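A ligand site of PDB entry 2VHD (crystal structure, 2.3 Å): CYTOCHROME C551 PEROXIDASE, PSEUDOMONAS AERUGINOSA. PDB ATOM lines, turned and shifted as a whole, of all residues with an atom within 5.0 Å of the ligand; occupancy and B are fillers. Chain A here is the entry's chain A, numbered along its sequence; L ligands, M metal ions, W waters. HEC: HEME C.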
ATOM      1  N   TRP A  94     -13.181 -23.000  16.809  1.00  0.00           N
ATOM      2  CA  TRP A  94     -13.779 -21.682  16.960  1.00  0.00           C
ATOM      3  C   TRP A  94     -15.150 -21.525  16.276  1.00  0.00           C
ATOM      4  O   TRP A  94     -15.956 -20.653  16.674  1.00  0.00           O
ATOM      5  CB  TRP A  94     -12.828 -20.577  16.467  1.00  0.00           C
ATOM      6  CG  TRP A  94     -11.624 -20.321  17.346  1.00  0.00           C
ATOM      7  CD1 TRP A  94     -10.351 -20.792  17.164  1.00  0.00           C
ATOM      8  CD2 TRP A  94     -11.591 -19.532  18.553  1.00  0.00           C
ATOM      9  NE1 TRP A  94      -9.546 -20.338  18.168  1.00  0.00           N
ATOM     10  CE2 TRP A  94     -10.272 -19.584  19.048  1.00  0.00           C
ATOM     11  CE3 TRP A  94     -12.560 -18.784  19.264  1.00  0.00           C
ATOM     12  CZ2 TRP A  94      -9.880 -18.911  20.218  1.00  0.00           C
ATOM     13  CZ3 TRP A  94     -12.155 -18.103  20.425  1.00  0.00           C
ATOM     14  CH2 TRP A  94     -10.831 -18.172  20.883  1.00  0.00           C
ATOM     15  N   PHE A 192     -18.539 -10.193  36.915  1.00  0.00           N
ATOM     16  CA  PHE A 192     -18.715 -11.126  35.819  1.00  0.00           C
ATOM     17  C   PHE A 192     -20.172 -11.544  35.663  1.00  0.00           C
ATOM     18  O   PHE A 192     -20.723 -11.546  34.545  1.00  0.00           O
ATOM     19  CB  PHE A 192     -17.833 -12.345  36.066  1.00  0.00           C
ATOM     20  CG  PHE A 192     -17.748 -13.286  34.904  1.00  0.00           C
ATOM     21  CD1 PHE A 192     -18.668 -14.325  34.759  1.00  0.00           C
ATOM     22  CD2 PHE A 192     -16.708 -13.177  33.974  1.00  0.00           C
ATOM     23  CE1 PHE A 192     -18.567 -15.224  33.686  1.00  0.00           C
ATOM     24  CE2 PHE A 192     -16.604 -14.045  32.896  1.00  0.00           C
ATOM     25  CZ  PHE A 192     -17.532 -15.080  32.756  1.00  0.00           C
ATOM     26  N   SER A 195     -22.761  -8.212  35.193  1.00  0.00           N
ATOM     27  CA  SER A 195     -22.592  -7.501  33.907  1.00  0.00           C
ATOM     28  C   SER A 195     -23.190  -8.280  32.751  1.00  0.00           C
ATOM     29  O   SER A 195     -23.361  -7.730  31.662  1.00  0.00           O
ATOM     30  CB  SER A 195     -21.125  -7.226  33.580  1.00  0.00           C
ATOM     31  OG  SER A 195     -20.422  -6.699  34.690  1.00  0.00           O
ATOM     32  N   GLY A 196     -23.490  -9.556  33.004  1.00  0.00           N
ATOM     33  CA  GLY A 196     -23.971 -10.476  31.962  1.00  0.00           C
ATOM     34  C   GLY A 196     -22.962 -11.364  31.220  1.00  0.00           C
ATOM     35  O   GLY A 196     -23.354 -12.055  30.283  1.00  0.00           O
ATOM     36  N   CYS A 197     -21.684 -11.352  31.607  1.00  0.00           N
ATOM     37  CA  CYS A 197     -20.665 -12.239  30.987  1.00  0.00           C
ATOM     38  C   CYS A 197     -21.059 -13.703  30.979  1.00  0.00           C
ATOM     39  O   CYS A 197     -20.849 -14.416  30.002  1.00  0.00           O
ATOM     40  CB  CYS A 197     -19.324 -12.160  31.729  1.00  0.00           C
ATOM     41  SG  CYS A 197     -18.659 -10.517  31.947  1.00  0.00           S
ATOM     42  N   CYS A 200     -23.145 -16.010  28.274  1.00  0.00           N
ATOM     43  CA  CYS A 200     -22.476 -16.731  27.181  1.00  0.00           C
ATOM     44  C   CYS A 200     -21.423 -17.687  27.715  1.00  0.00           C
ATOM     45  O   CYS A 200     -21.192 -18.748  27.144  1.00  0.00           O
ATOM     46  CB  CYS A 200     -21.821 -15.751  26.189  1.00  0.00           C
ATOM     47  SG  CYS A 200     -22.949 -14.491  25.463  1.00  0.00           S
ATOM     48  N   HIS A 201     -20.782 -17.286  28.810  1.00  0.00           N
ATOM     49  CA  HIS A 201     -19.775 -18.103  29.472  1.00  0.00           C
ATOM     50  C   HIS A 201     -20.366 -18.736  30.730  1.00  0.00           C
ATOM     51  O   HIS A 201     -20.227 -18.194  31.820  1.00  0.00           O
ATOM     52  CB  HIS A 201     -18.564 -17.237  29.874  1.00  0.00           C
ATOM     53  CG  HIS A 201     -17.931 -16.475  28.746  1.00  0.00           C
ATOM     54  ND1 HIS A 201     -17.109 -17.075  27.820  1.00  0.00           N
ATOM     55  CD2 HIS A 201     -17.988 -15.158  28.415  1.00  0.00           C
ATOM     56  CE1 HIS A 201     -16.691 -16.159  26.963  1.00  0.00           C
ATOM     57  NE2 HIS A 201     -17.201 -14.992  27.301  1.00  0.00           N
ATOM     58  N   PHE A 212     -22.115 -16.940  19.224  1.00  0.00           N
ATOM     59  CA  PHE A 212     -22.667 -15.592  19.289  1.00  0.00           C
ATOM     60  C   PHE A 212     -21.882 -14.657  18.402  1.00  0.00           C
ATOM     61  O   PHE A 212     -20.698 -14.902  18.148  1.00  0.00           O
ATOM     62  CB  PHE A 212     -22.574 -15.040  20.702  1.00  0.00           C
ATOM     63  CG  PHE A 212     -23.272 -15.869  21.709  1.00  0.00           C
ATOM     64  CD1 PHE A 212     -24.647 -15.716  21.922  1.00  0.00           C
ATOM     65  CD2 PHE A 212     -22.558 -16.782  22.470  1.00  0.00           C
ATOM     66  CE1 PHE A 212     -25.299 -16.492  22.883  1.00  0.00           C
ATOM     67  CE2 PHE A 212     -23.191 -17.560  23.401  1.00  0.00           C
ATOM     68  CZ  PHE A 212     -24.559 -17.401  23.617  1.00  0.00           C
ATOM     69  N   PRO A 213     -22.514 -13.540  17.952  1.00  0.00           N
ATOM     70  CA  PRO A 213     -21.698 -12.583  17.221  1.00  0.00           C
ATOM     71  C   PRO A 213     -20.549 -12.096  18.098  1.00  0.00           C
ATOM     72  O   PRO A 213     -20.744 -11.854  19.299  1.00  0.00           O
ATOM     73  CB  PRO A 213     -22.672 -11.442  16.926  1.00  0.00           C
ATOM     74  CG  PRO A 213     -24.035 -12.075  17.010  1.00  0.00           C
ATOM     75  CD  PRO A 213     -23.909 -13.104  18.082  1.00  0.00           C
ATOM     76  N   PHE A 214     -19.357 -11.994  17.529  1.00  0.00           N
ATOM     77  CA  PHE A 214     -18.298 -11.257  18.202  1.00  0.00           C
ATOM     78  C   PHE A 214     -18.660  -9.775  17.943  1.00  0.00           C
ATOM     79  O   PHE A 214     -18.323  -9.191  16.907  1.00  0.00           O
ATOM     80  CB  PHE A 214     -16.932 -11.679  17.668  1.00  0.00           C
ATOM     81  CG  PHE A 214     -15.777 -11.108  18.429  1.00  0.00           C
ATOM     82  CD1 PHE A 214     -15.971 -10.317  19.568  1.00  0.00           C
ATOM     83  CD2 PHE A 214     -14.464 -11.386  18.029  1.00  0.00           C
ATOM     84  CE1 PHE A 214     -14.879  -9.791  20.273  1.00  0.00           C
ATOM     85  CE2 PHE A 214     -13.356 -10.869  18.725  1.00  0.00           C
ATOM     86  CZ  PHE A 214     -13.556 -10.097  19.852  1.00  0.00           C
ATOM     87  N   LEU A 216     -22.079  -8.620  19.674  1.00  0.00           N
ATOM     88  CA  LEU A 216     -23.533  -8.613  19.887  1.00  0.00           C
ATOM     89  C   LEU A 216     -24.098  -7.168  19.961  1.00  0.00           C
ATOM     90  O   LEU A 216     -25.232  -6.884  19.506  1.00  0.00           O
ATOM     91  CB  LEU A 216     -23.897  -9.429  21.136  1.00  0.00           C
ATOM     92  CG  LEU A 216     -25.402  -9.529  21.481  1.00  0.00           C
ATOM     93  CD1 LEU A 216     -26.248 -10.088  20.326  1.00  0.00           C
ATOM     94  CD2 LEU A 216     -25.643 -10.327  22.782  1.00  0.00           C
ATOM     95  N   PHE A 245     -19.002 -16.497  16.479  1.00  0.00           N
ATOM     96  CA  PHE A 245     -18.017 -17.497  16.969  1.00  0.00           C
ATOM     97  C   PHE A 245     -18.528 -18.270  18.177  1.00  0.00           C
ATOM     98  O   PHE A 245     -19.475 -17.857  18.812  1.00  0.00           O
ATOM     99  CB  PHE A 245     -16.660 -16.860  17.258  1.00  0.00           C
ATOM    100  CG  PHE A 245     -15.972 -16.341  16.014  1.00  0.00           C
ATOM    101  CD1 PHE A 245     -16.336 -15.115  15.455  1.00  0.00           C
ATOM    102  CD2 PHE A 245     -14.994 -17.100  15.392  1.00  0.00           C
ATOM    103  CE1 PHE A 245     -15.705 -14.645  14.297  1.00  0.00           C
ATOM    104  CE2 PHE A 245     -14.362 -16.635  14.243  1.00  0.00           C
ATOM    105  CZ  PHE A 245     -14.708 -15.419  13.699  1.00  0.00           C
ATOM    106  N   ARG A 246     -17.941 -19.434  18.431  1.00  0.00           N
ATOM    107  CA  ARG A 246     -18.272 -20.186  19.669  1.00  0.00           C
ATOM    108  C   ARG A 246     -17.828 -19.360  20.874  1.00  0.00           C
ATOM    109  O   ARG A 246     -16.710 -18.863  20.877  1.00  0.00           O
ATOM    110  CB  ARG A 246     -17.639 -21.575  19.646  1.00  0.00           C
ATOM    111  CG  ARG A 246     -17.998 -22.431  20.879  1.00  0.00           C
ATOM    112  CD  ARG A 246     -17.137 -23.676  21.013  1.00  0.00           C
ATOM    113  NE  ARG A 246     -15.745 -23.391  21.347  1.00  0.00           N
ATOM    114  CZ  ARG A 246     -14.820 -24.317  21.604  1.00  0.00           C
ATOM    115  NH1 ARG A 246     -15.134 -25.624  21.543  1.00  0.00           N
ATOM    116  NH2 ARG A 246     -13.583 -23.943  21.880  1.00  0.00           N
ATOM    117  N   ALA A 247     -18.716 -19.155  21.858  1.00  0.00           N
ATOM    118  CA  ALA A 247     -18.303 -18.520  23.122  1.00  0.00           C
ATOM    119  C   ALA A 247     -17.097 -19.290  23.669  1.00  0.00           C
ATOM    120  O   ALA A 247     -17.142 -20.499  23.835  1.00  0.00           O
ATOM    121  CB  ALA A 247     -19.441 -18.498  24.148  1.00  0.00           C
ATOM    122  N   ALA A 248     -15.992 -18.585  23.892  1.00  0.00           N
ATOM    123  CA  ALA A 248     -14.753 -19.186  24.280  1.00  0.00           C
ATOM    124  C   ALA A 248     -14.866 -19.755  25.703  1.00  0.00           C
ATOM    125  O   ALA A 248     -15.334 -19.086  26.612  1.00  0.00           O
ATOM    126  CB  ALA A 248     -13.619 -18.178  24.178  1.00  0.00           C
ATOM    127  N   PRO A 249     -14.456 -21.014  25.898  1.00  0.00           N
ATOM    128  CA  PRO A 249     -14.462 -21.515  27.276  1.00  0.00           C
ATOM    129  C   PRO A 249     -13.315 -20.870  28.077  1.00  0.00           C
ATOM    130  O   PRO A 249     -12.178 -20.777  27.599  1.00  0.00           O
ATOM    131  CB  PRO A 249     -14.252 -23.030  27.108  1.00  0.00           C
ATOM    132  CG  PRO A 249     -13.559 -23.187  25.763  1.00  0.00           C
ATOM    133  CD  PRO A 249     -13.981 -22.021  24.914  1.00  0.00           C
ATOM    134  N   LEU A 250     -13.620 -20.405  29.282  1.00  0.00           N
ATOM    135  CA  LEU A 250     -12.696 -19.524  29.981  1.00  0.00           C
ATOM    136  C   LEU A 250     -11.710 -20.222  30.939  1.00  0.00           C
ATOM    137  O   LEU A 250     -10.762 -19.611  31.434  1.00  0.00           O
ATOM    138  CB  LEU A 250     -13.439 -18.352  30.625  1.00  0.00           C
ATOM    139  CG  LEU A 250     -13.988 -17.321  29.645  1.00  0.00           C
ATOM    140  CD1 LEU A 250     -14.598 -16.129  30.376  1.00  0.00           C
ATOM    141  CD2 LEU A 250     -12.949 -16.838  28.679  1.00  0.00           C
ATOM    142  N   VAL A 253      -7.838 -19.652  31.085  1.00  0.00           N
ATOM    143  CA  VAL A 253      -7.662 -18.451  30.237  1.00  0.00           C
ATOM    144  C   VAL A 253      -6.432 -17.617  30.637  1.00  0.00           C
ATOM    145  O   VAL A 253      -5.799 -16.996  29.781  1.00  0.00           O
ATOM    146  CB  VAL A 253      -8.929 -17.587  30.246  1.00  0.00           C
ATOM    147  CG1 VAL A 253      -9.189 -17.017  31.675  1.00  0.00           C
ATOM    148  CG2 VAL A 253      -8.885 -16.474  29.127  1.00  0.00           C
ATOM    149  N   THR A 256      -3.177 -19.064  28.574  1.00  0.00           N
ATOM    150  CA  THR A 256      -3.298 -19.241  27.143  1.00  0.00           C
ATOM    151  C   THR A 256      -3.360 -17.905  26.358  1.00  0.00           C
ATOM    152  O   THR A 256      -3.996 -17.838  25.291  1.00  0.00           O
ATOM    153  CB  THR A 256      -4.565 -20.121  26.816  1.00  0.00           C
ATOM    154  OG1 THR A 256      -5.751 -19.462  27.272  1.00  0.00           O
ATOM    155  CG2 THR A 256      -4.477 -21.493  27.510  1.00  0.00           C
ATOM    156  N   PRO A 258      -2.044 -15.305  23.671  1.00  0.00           N
ATOM    157  CA  PRO A 258      -3.000 -14.248  23.449  1.00  0.00           C
ATOM    158  C   PRO A 258      -4.457 -14.690  23.252  1.00  0.00           C
ATOM    159  O   PRO A 258      -4.729 -15.885  23.125  1.00  0.00           O
ATOM    160  CB  PRO A 258      -2.461 -13.553  22.194  1.00  0.00           C
ATOM    161  CG  PRO A 258      -1.743 -14.606  21.453  1.00  0.00           C
ATOM    162  CD  PRO A 258      -1.249 -15.592  22.450  1.00  0.00           C
ATOM    163  N   TYR A 259      -5.375 -13.728  23.142  1.00  0.00           N
ATOM    164  CA  TYR A 259      -6.787 -13.994  23.207  1.00  0.00           C
ATOM    165  C   TYR A 259      -7.611 -13.727  21.957  1.00  0.00           C
ATOM    166  O   TYR A 259      -7.138 -13.094  21.003  1.00  0.00           O
ATOM    167  CB  TYR A 259      -7.364 -13.248  24.398  1.00  0.00           C
ATOM    168  CG  TYR A 259      -6.621 -13.645  25.648  1.00  0.00           C
ATOM    169  CD1 TYR A 259      -6.764 -14.922  26.154  1.00  0.00           C
ATOM    170  CD2 TYR A 259      -5.740 -12.741  26.297  1.00  0.00           C
ATOM    171  CE1 TYR A 259      -6.064 -15.318  27.313  1.00  0.00           C
ATOM    172  CE2 TYR A 259      -5.036 -13.125  27.451  1.00  0.00           C
ATOM    173  CZ  TYR A 259      -5.217 -14.425  27.961  1.00  0.00           C
ATOM    174  OH  TYR A 259      -4.576 -14.830  29.100  1.00  0.00           O
ATOM    175  N   PHE A 260      -8.853 -14.231  21.997  1.00  0.00           N
ATOM    176  CA  PHE A 260      -9.745 -14.376  20.842  1.00  0.00           C
ATOM    177  C   PHE A 260      -9.162 -15.256  19.729  1.00  0.00           C
ATOM    178  O   PHE A 260      -7.976 -15.671  19.800  1.00  0.00           O
ATOM    179  CB  PHE A 260     -10.227 -12.998  20.324  1.00  0.00           C
ATOM    180  CG  PHE A 260     -10.629 -12.092  21.422  1.00  0.00           C
ATOM    181  CD1 PHE A 260     -11.710 -12.417  22.246  1.00  0.00           C
ATOM    182  CD2 PHE A 260      -9.874 -10.931  21.694  1.00  0.00           C
ATOM    183  CE1 PHE A 260     -12.053 -11.596  23.287  1.00  0.00           C
ATOM    184  CE2 PHE A 260     -10.192 -10.088  22.732  1.00  0.00           C
ATOM    185  CZ  PHE A 260     -11.283 -10.409  23.537  1.00  0.00           C
ATOM    186  N   HIS A 261     -10.011 -15.553  18.732  1.00  0.00           N
ATOM    187  CA  HIS A 261      -9.637 -16.498  17.674  1.00  0.00           C
ATOM    188  C   HIS A 261      -8.459 -15.978  16.893  1.00  0.00           C
ATOM    189  O   HIS A 261      -7.703 -16.764  16.306  1.00  0.00           O
ATOM    190  CB  HIS A 261     -10.822 -16.810  16.753  1.00  0.00           C
ATOM    191  CG  HIS A 261     -11.285 -15.627  15.949  1.00  0.00           C
ATOM    192  ND1 HIS A 261     -12.244 -14.754  16.400  1.00  0.00           N
ATOM    193  CD2 HIS A 261     -10.927 -15.197  14.715  1.00  0.00           C
ATOM    194  CE1 HIS A 261     -12.457 -13.826  15.483  1.00  0.00           C
ATOM    195  NE2 HIS A 261     -11.661 -14.067  14.454  1.00  0.00           N
ATOM    196  N   LEU A 268      -4.971  -9.748  29.304  1.00  0.00           N
ATOM    197  CA  LEU A 268      -6.259 -10.230  29.700  1.00  0.00           C
ATOM    198  C   LEU A 268      -7.190  -9.067  30.052  1.00  0.00           C
ATOM    199  O   LEU A 268      -8.394  -9.092  29.753  1.00  0.00           O
ATOM    200  CB  LEU A 268      -6.048 -11.183  30.896  1.00  0.00           C
ATOM    201  CG  LEU A 268      -7.119 -12.200  31.299  1.00  0.00           C
ATOM    202  CD1 LEU A 268      -7.822 -12.842  30.072  1.00  0.00           C
ATOM    203  CD2 LEU A 268      -6.470 -13.257  32.231  1.00  0.00           C
ATOM    204  N   ALA A 271      -8.777  -7.874  27.049  1.00  0.00           N
ATOM    205  CA  ALA A 271      -9.723  -8.828  26.476  1.00  0.00           C
ATOM    206  C   ALA A 271     -11.058  -8.671  27.177  1.00  0.00           C
ATOM    207  O   ALA A 271     -12.106  -8.678  26.554  1.00  0.00           O
ATOM    208  CB  ALA A 271      -9.189 -10.273  26.629  1.00  0.00           C
ATOM    209  N   VAL A 272     -10.991  -8.578  28.498  1.00  0.00           N
ATOM    210  CA  VAL A 272     -12.144  -8.265  29.335  1.00  0.00           C
ATOM    211  C   VAL A 272     -12.833  -6.953  28.896  1.00  0.00           C
ATOM    212  O   VAL A 272     -14.052  -6.917  28.790  1.00  0.00           O
ATOM    213  CB  VAL A 272     -11.779  -8.234  30.853  1.00  0.00           C
ATOM    214  CG1 VAL A 272     -12.962  -7.716  31.690  1.00  0.00           C
ATOM    215  CG2 VAL A 272     -11.364  -9.604  31.339  1.00  0.00           C
ATOM    216  N   MET A 275     -14.523  -7.210  25.607  1.00  0.00           N
ATOM    217  CA  MET A 275     -15.734  -8.025  25.734  1.00  0.00           C
ATOM    218  C   MET A 275     -16.904  -7.283  26.343  1.00  0.00           C
ATOM    219  O   MET A 275     -18.037  -7.483  25.908  1.00  0.00           O
ATOM    220  CB  MET A 275     -15.471  -9.331  26.490  1.00  0.00           C
ATOM    221  CG  MET A 275     -14.939 -10.463  25.617  1.00  0.00           C
ATOM    222  SD  MET A 275     -16.277 -11.458  24.928  1.00  0.00           S
ATOM    223  CE  MET A 275     -16.000 -11.202  23.183  1.00  0.00           C
ATOM    224  N   GLY A 276     -16.647  -6.425  27.346  1.00  0.00           N
ATOM    225  CA  GLY A 276     -17.698  -5.525  27.858  1.00  0.00           C
ATOM    226  C   GLY A 276     -18.294  -4.618  26.776  1.00  0.00           C
ATOM    227  O   GLY A 276     -19.498  -4.462  26.639  1.00  0.00           O
ATOM    228  N   GLN A 279     -19.827  -6.923  23.649  1.00  0.00           N
ATOM    229  CA  GLN A 279     -20.883  -7.891  23.900  1.00  0.00           C
ATOM    230  C   GLN A 279     -21.980  -7.337  24.795  1.00  0.00           C
ATOM    231  O   GLN A 279     -23.136  -7.828  24.767  1.00  0.00           O
ATOM    232  CB  GLN A 279     -20.305  -9.190  24.491  1.00  0.00           C
ATOM    233  CG  GLN A 279     -19.239  -9.895  23.632  1.00  0.00           C
ATOM    234  CD  GLN A 279     -19.770 -10.360  22.287  1.00  0.00           C
ATOM    235  OE1 GLN A 279     -19.906  -9.572  21.357  1.00  0.00           O
ATOM    236  NE2 GLN A 279     -20.006 -11.649  22.162  1.00  0.00           N
ATOM    237  N   LEU A 280     -21.615  -6.317  25.571  1.00  0.00           N
ATOM    238  CA  LEU A 280     -22.489  -5.783  26.608  1.00  0.00           C
ATOM    239  C   LEU A 280     -22.787  -4.280  26.476  1.00  0.00           C
ATOM    240  O   LEU A 280     -23.724  -3.784  27.129  1.00  0.00           O
ATOM    241  CB  LEU A 280     -21.932  -6.114  27.987  1.00  0.00           C
ATOM    242  CG  LEU A 280     -21.832  -7.606  28.349  1.00  0.00           C
ATOM    243  CD1 LEU A 280     -21.018  -7.752  29.611  1.00  0.00           C
ATOM    244  CD2 LEU A 280     -23.252  -8.242  28.516  1.00  0.00           C
ATOM    245  N   LEU A 284     -16.354  -1.048  31.186  1.00  0.00           N
ATOM    246  CA  LEU A 284     -16.143  -1.470  32.553  1.00  0.00           C
ATOM    247  C   LEU A 284     -15.186  -0.514  33.248  1.00  0.00           C
ATOM    248  O   LEU A 284     -14.201  -0.087  32.660  1.00  0.00           O
ATOM    249  CB  LEU A 284     -15.595  -2.918  32.603  1.00  0.00           C
ATOM    250  CG  LEU A 284     -16.423  -4.036  31.956  1.00  0.00           C
ATOM    251  CD1 LEU A 284     -15.602  -5.298  31.740  1.00  0.00           C
ATOM    252  CD2 LEU A 284     -17.683  -4.329  32.761  1.00  0.00           C
ATOM    253  N   ILE A 292     -12.461  -8.640  37.568  1.00  0.00           N
ATOM    254  CA  ILE A 292     -12.745  -9.724  36.622  1.00  0.00           C
ATOM    255  C   ILE A 292     -11.462 -10.491  36.197  1.00  0.00           C
ATOM    256  O   ILE A 292     -11.474 -11.712  36.127  1.00  0.00           O
ATOM    257  CB  ILE A 292     -13.582  -9.260  35.388  1.00  0.00           C
ATOM    258  CG1 ILE A 292     -14.946  -8.709  35.838  1.00  0.00           C
ATOM    259  CG2 ILE A 292     -13.777 -10.429  34.415  1.00  0.00           C
ATOM    260  CD1 ILE A 292     -15.812  -8.092  34.703  1.00  0.00           C
ATOM    261  N   LEU A 296     -10.894 -14.458  36.686  1.00  0.00           N
ATOM    262  CA  LEU A 296     -10.393 -15.333  35.629  1.00  0.00           C
ATOM    263  C   LEU A 296      -9.133 -16.117  36.021  1.00  0.00           C
ATOM    264  O   LEU A 296      -8.922 -17.205  35.510  1.00  0.00           O
ATOM    265  CB  LEU A 296     -10.160 -14.577  34.338  1.00  0.00           C
ATOM    266  CG  LEU A 296     -11.402 -13.935  33.733  1.00  0.00           C
ATOM    267  CD1 LEU A 296     -11.013 -13.220  32.433  1.00  0.00           C
ATOM    268  CD2 LEU A 296     -12.618 -14.913  33.587  1.00  0.00           C
HETATM  269 FE   HEC L   1     -16.725 -13.395  26.105  1.00  0.00          FE
HETATM  270  CHA HEC L   1     -14.243 -14.693  24.153  1.00  0.00           C
HETATM  271  CHB HEC L   1     -14.376 -12.683  28.553  1.00  0.00           C
HETATM  272  CHC HEC L   1     -19.055 -11.491  27.859  1.00  0.00           C
HETATM  273  CHD HEC L   1     -19.179 -14.468  24.090  1.00  0.00           C
HETATM  274  NA  HEC L   1     -14.647 -13.650  26.331  1.00  0.00           N
HETATM  275  C1A HEC L   1     -13.799 -14.199  25.374  1.00  0.00           C
HETATM  276  C2A HEC L   1     -12.423 -14.132  25.904  1.00  0.00           C
HETATM  277  C3A HEC L   1     -12.496 -13.586  27.122  1.00  0.00           C
HETATM  278  C4A HEC L   1     -13.886 -13.284  27.417  1.00  0.00           C
HETATM  279  CMA HEC L   1     -11.338 -13.314  28.081  1.00  0.00           C
HETATM  280  CAA HEC L   1     -11.117 -14.615  25.228  1.00  0.00           C
HETATM  281  CBA HEC L   1     -11.042 -16.139  25.412  1.00  0.00           C
HETATM  282  CGA HEC L   1      -9.908 -16.793  24.699  1.00  0.00           C
HETATM  283  O1A HEC L   1      -9.650 -17.946  25.057  1.00  0.00           O
HETATM  284  O2A HEC L   1      -9.247 -16.243  23.788  1.00  0.00           O
HETATM  285  NB  HEC L   1     -16.701 -12.323  27.867  1.00  0.00           N
HETATM  286  C1B HEC L   1     -15.626 -12.103  28.682  1.00  0.00           C
HETATM  287  C2B HEC L   1     -16.015 -11.136  29.697  1.00  0.00           C
HETATM  288  C3B HEC L   1     -17.327 -10.815  29.498  1.00  0.00           C
HETATM  289  C4B HEC L   1     -17.768 -11.536  28.340  1.00  0.00           C
HETATM  290  CMB HEC L   1     -15.063 -10.672  30.840  1.00  0.00           C
HETATM  291  CAB HEC L   1     -18.275  -9.866  30.296  1.00  0.00           C
HETATM  292  CBB HEC L   1     -17.606  -8.525  30.634  1.00  0.00           C
HETATM  293  NC  HEC L   1     -18.769 -13.048  26.035  1.00  0.00           N
HETATM  294  C1C HEC L   1     -19.540 -12.207  26.799  1.00  0.00           C
HETATM  295  C2C HEC L   1     -20.916 -12.285  26.322  1.00  0.00           C
HETATM  296  C3C HEC L   1     -20.907 -13.033  25.185  1.00  0.00           C
HETATM  297  C4C HEC L   1     -19.584 -13.573  25.045  1.00  0.00           C
HETATM  298  CMC HEC L   1     -22.033 -11.354  26.867  1.00  0.00           C
HETATM  299  CAC HEC L   1     -22.040 -13.478  24.225  1.00  0.00           C
HETATM  300  CBC HEC L   1     -23.037 -12.421  23.764  1.00  0.00           C
HETATM  301  ND  HEC L   1     -16.722 -14.504  24.423  1.00  0.00           N
HETATM  302  C1D HEC L   1     -17.886 -14.673  23.671  1.00  0.00           C
HETATM  303  C2D HEC L   1     -17.522 -15.106  22.355  1.00  0.00           C
HETATM  304  C3D HEC L   1     -15.988 -15.189  22.370  1.00  0.00           C
HETATM  305  C4D HEC L   1     -15.559 -14.780  23.696  1.00  0.00           C
HETATM  306  CMD HEC L   1     -18.476 -15.430  21.174  1.00  0.00           C
HETATM  307  CAD HEC L   1     -15.130 -15.608  21.169  1.00  0.00           C
HETATM  308  CBD HEC L   1     -14.882 -14.343  20.351  1.00  0.00           C
HETATM  309  CGD HEC L   1     -13.810 -14.655  19.320  1.00  0.00           C
HETATM  310  O1D HEC L   1     -12.595 -14.763  19.685  1.00  0.00           O
HETATM  311  O2D HEC L   1     -14.190 -14.795  18.124  1.00  0.00           O
HETATM  312 CA    CA M   1      -5.136 -18.111  23.330  1.00  0.00          CA
HETATM  313  O   HOH W   1      -6.923 -18.204  25.062  1.00  0.00           O
HETATM  314  O   HOH W   2      -7.499 -17.482  22.420  1.00  0.00           O
HETATM  315  O   HOH W   3     -10.040 -19.534  27.303  1.00  0.00           O
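Merely in contact with the ligand: Trp 94 (3.4 Å), Gly 196 (3.7 Å), Phe 212 (3.7 Å), Phe 214 (3.4 Å), Leu 216 (3.5 Å), Phe 245 (3.2 Å), Arg 246 (3.6 Å), Ala 247 (3.6 Å), Ala 248 (3.5 Å), Leu 250 (3.6 Å), Tyr 259 (3.4 Å), Ala 271 (3.997 Å), Val 272 (3.7 Å), Gln 279 (3.4 Å), Leu 280 (3.5 Å), Leu 284 (3.96 Å) and Ile 292 (3.8 Å). Hydrophobic or aromatic side chains that line the ligand: Trp 94, His 201, Phe 212, Phe 214, Leu 216, Phe 245, Ala 248, Leu 250, Tyr 259, Phe 260, His 261, Ala 271, Val 272, Met 275, Leu 280, Leu 284 and Ile 292. Of the 33 residues printed, 23 come within 4 Å of the ligand. The nearest printed residue that does not touch the ligand is Gly 276 (4.02 Å).
A ring nitrogen (ND1) of His 261 is in hydrogen-bond range of an oxygen (O2D) of the ligand (2.6 Å). FE of the ligand is bound by NE2 of His 201, 2.1 Å away. The side-chain sulfur (SD) of Met 275 is bound to an iron atom (FE) of the ligand. The backbone NH (N) of His 261 sits at hydrogen-bond distance from an oxygen (O1D) of the ligand (2.9 Å). The backbone NH (N) of Phe 260 lies within hydrogen-bond range of an oxygen (O2A) of the ligand, 2.7 Å away. The side-chain sulfur of Cys 197 is covalently linked to a carbon (CAB) of the ligand. SG of Cys 200 is covalently linked to CAC of the ligand.
Water W2 lies within hydrogen-bond range of an oxygen (O2A) of the ligand (2.5 Å) and the backbone carbonyl oxygen (O) of Phe 260 (3.2 Å). Water W1 lies within hydrogen-bond range of an oxygen (O1A) of the ligand (2.7 Å) and the side-chain hydroxyl (OG1) of Thr 256 (2.8 Å). Water W3 bridges O of Pro 249 (2.5 Å) and O1A of the ligand (2.8 Å).
The backbone carbonyl oxygen (O) of Trp 94 is in hydrogen-bond range of the backbone NH (N) of Arg 246 (2.9 Å). O of Phe 245 sits at hydrogen-bond distance from N of Phe 212 (2.8 Å). The side-chain amide oxygen of Gln 279 is in hydrogen-bond range of the backbone NH of Leu 216. The backbone carbonyl oxygen of Ala 248 lies within hydrogen-bond range of a ring nitrogen (ND1) of His 201 (2.9 Å). The backbone carbonyl oxygen (O) of Pro 213 lies within hydrogen-bond range of the side-chain amide nitrogen (NE2) of Gln 279 (3.0 Å). N of Cys 197 lies within hydrogen-bond range of O of Phe 192 (3.1 Å). The backbone carbonyl oxygen (O) of Val 253 lies within hydrogen-bond range of the side-chain hydroxyl (OH) of Tyr 259 (2.6 Å).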
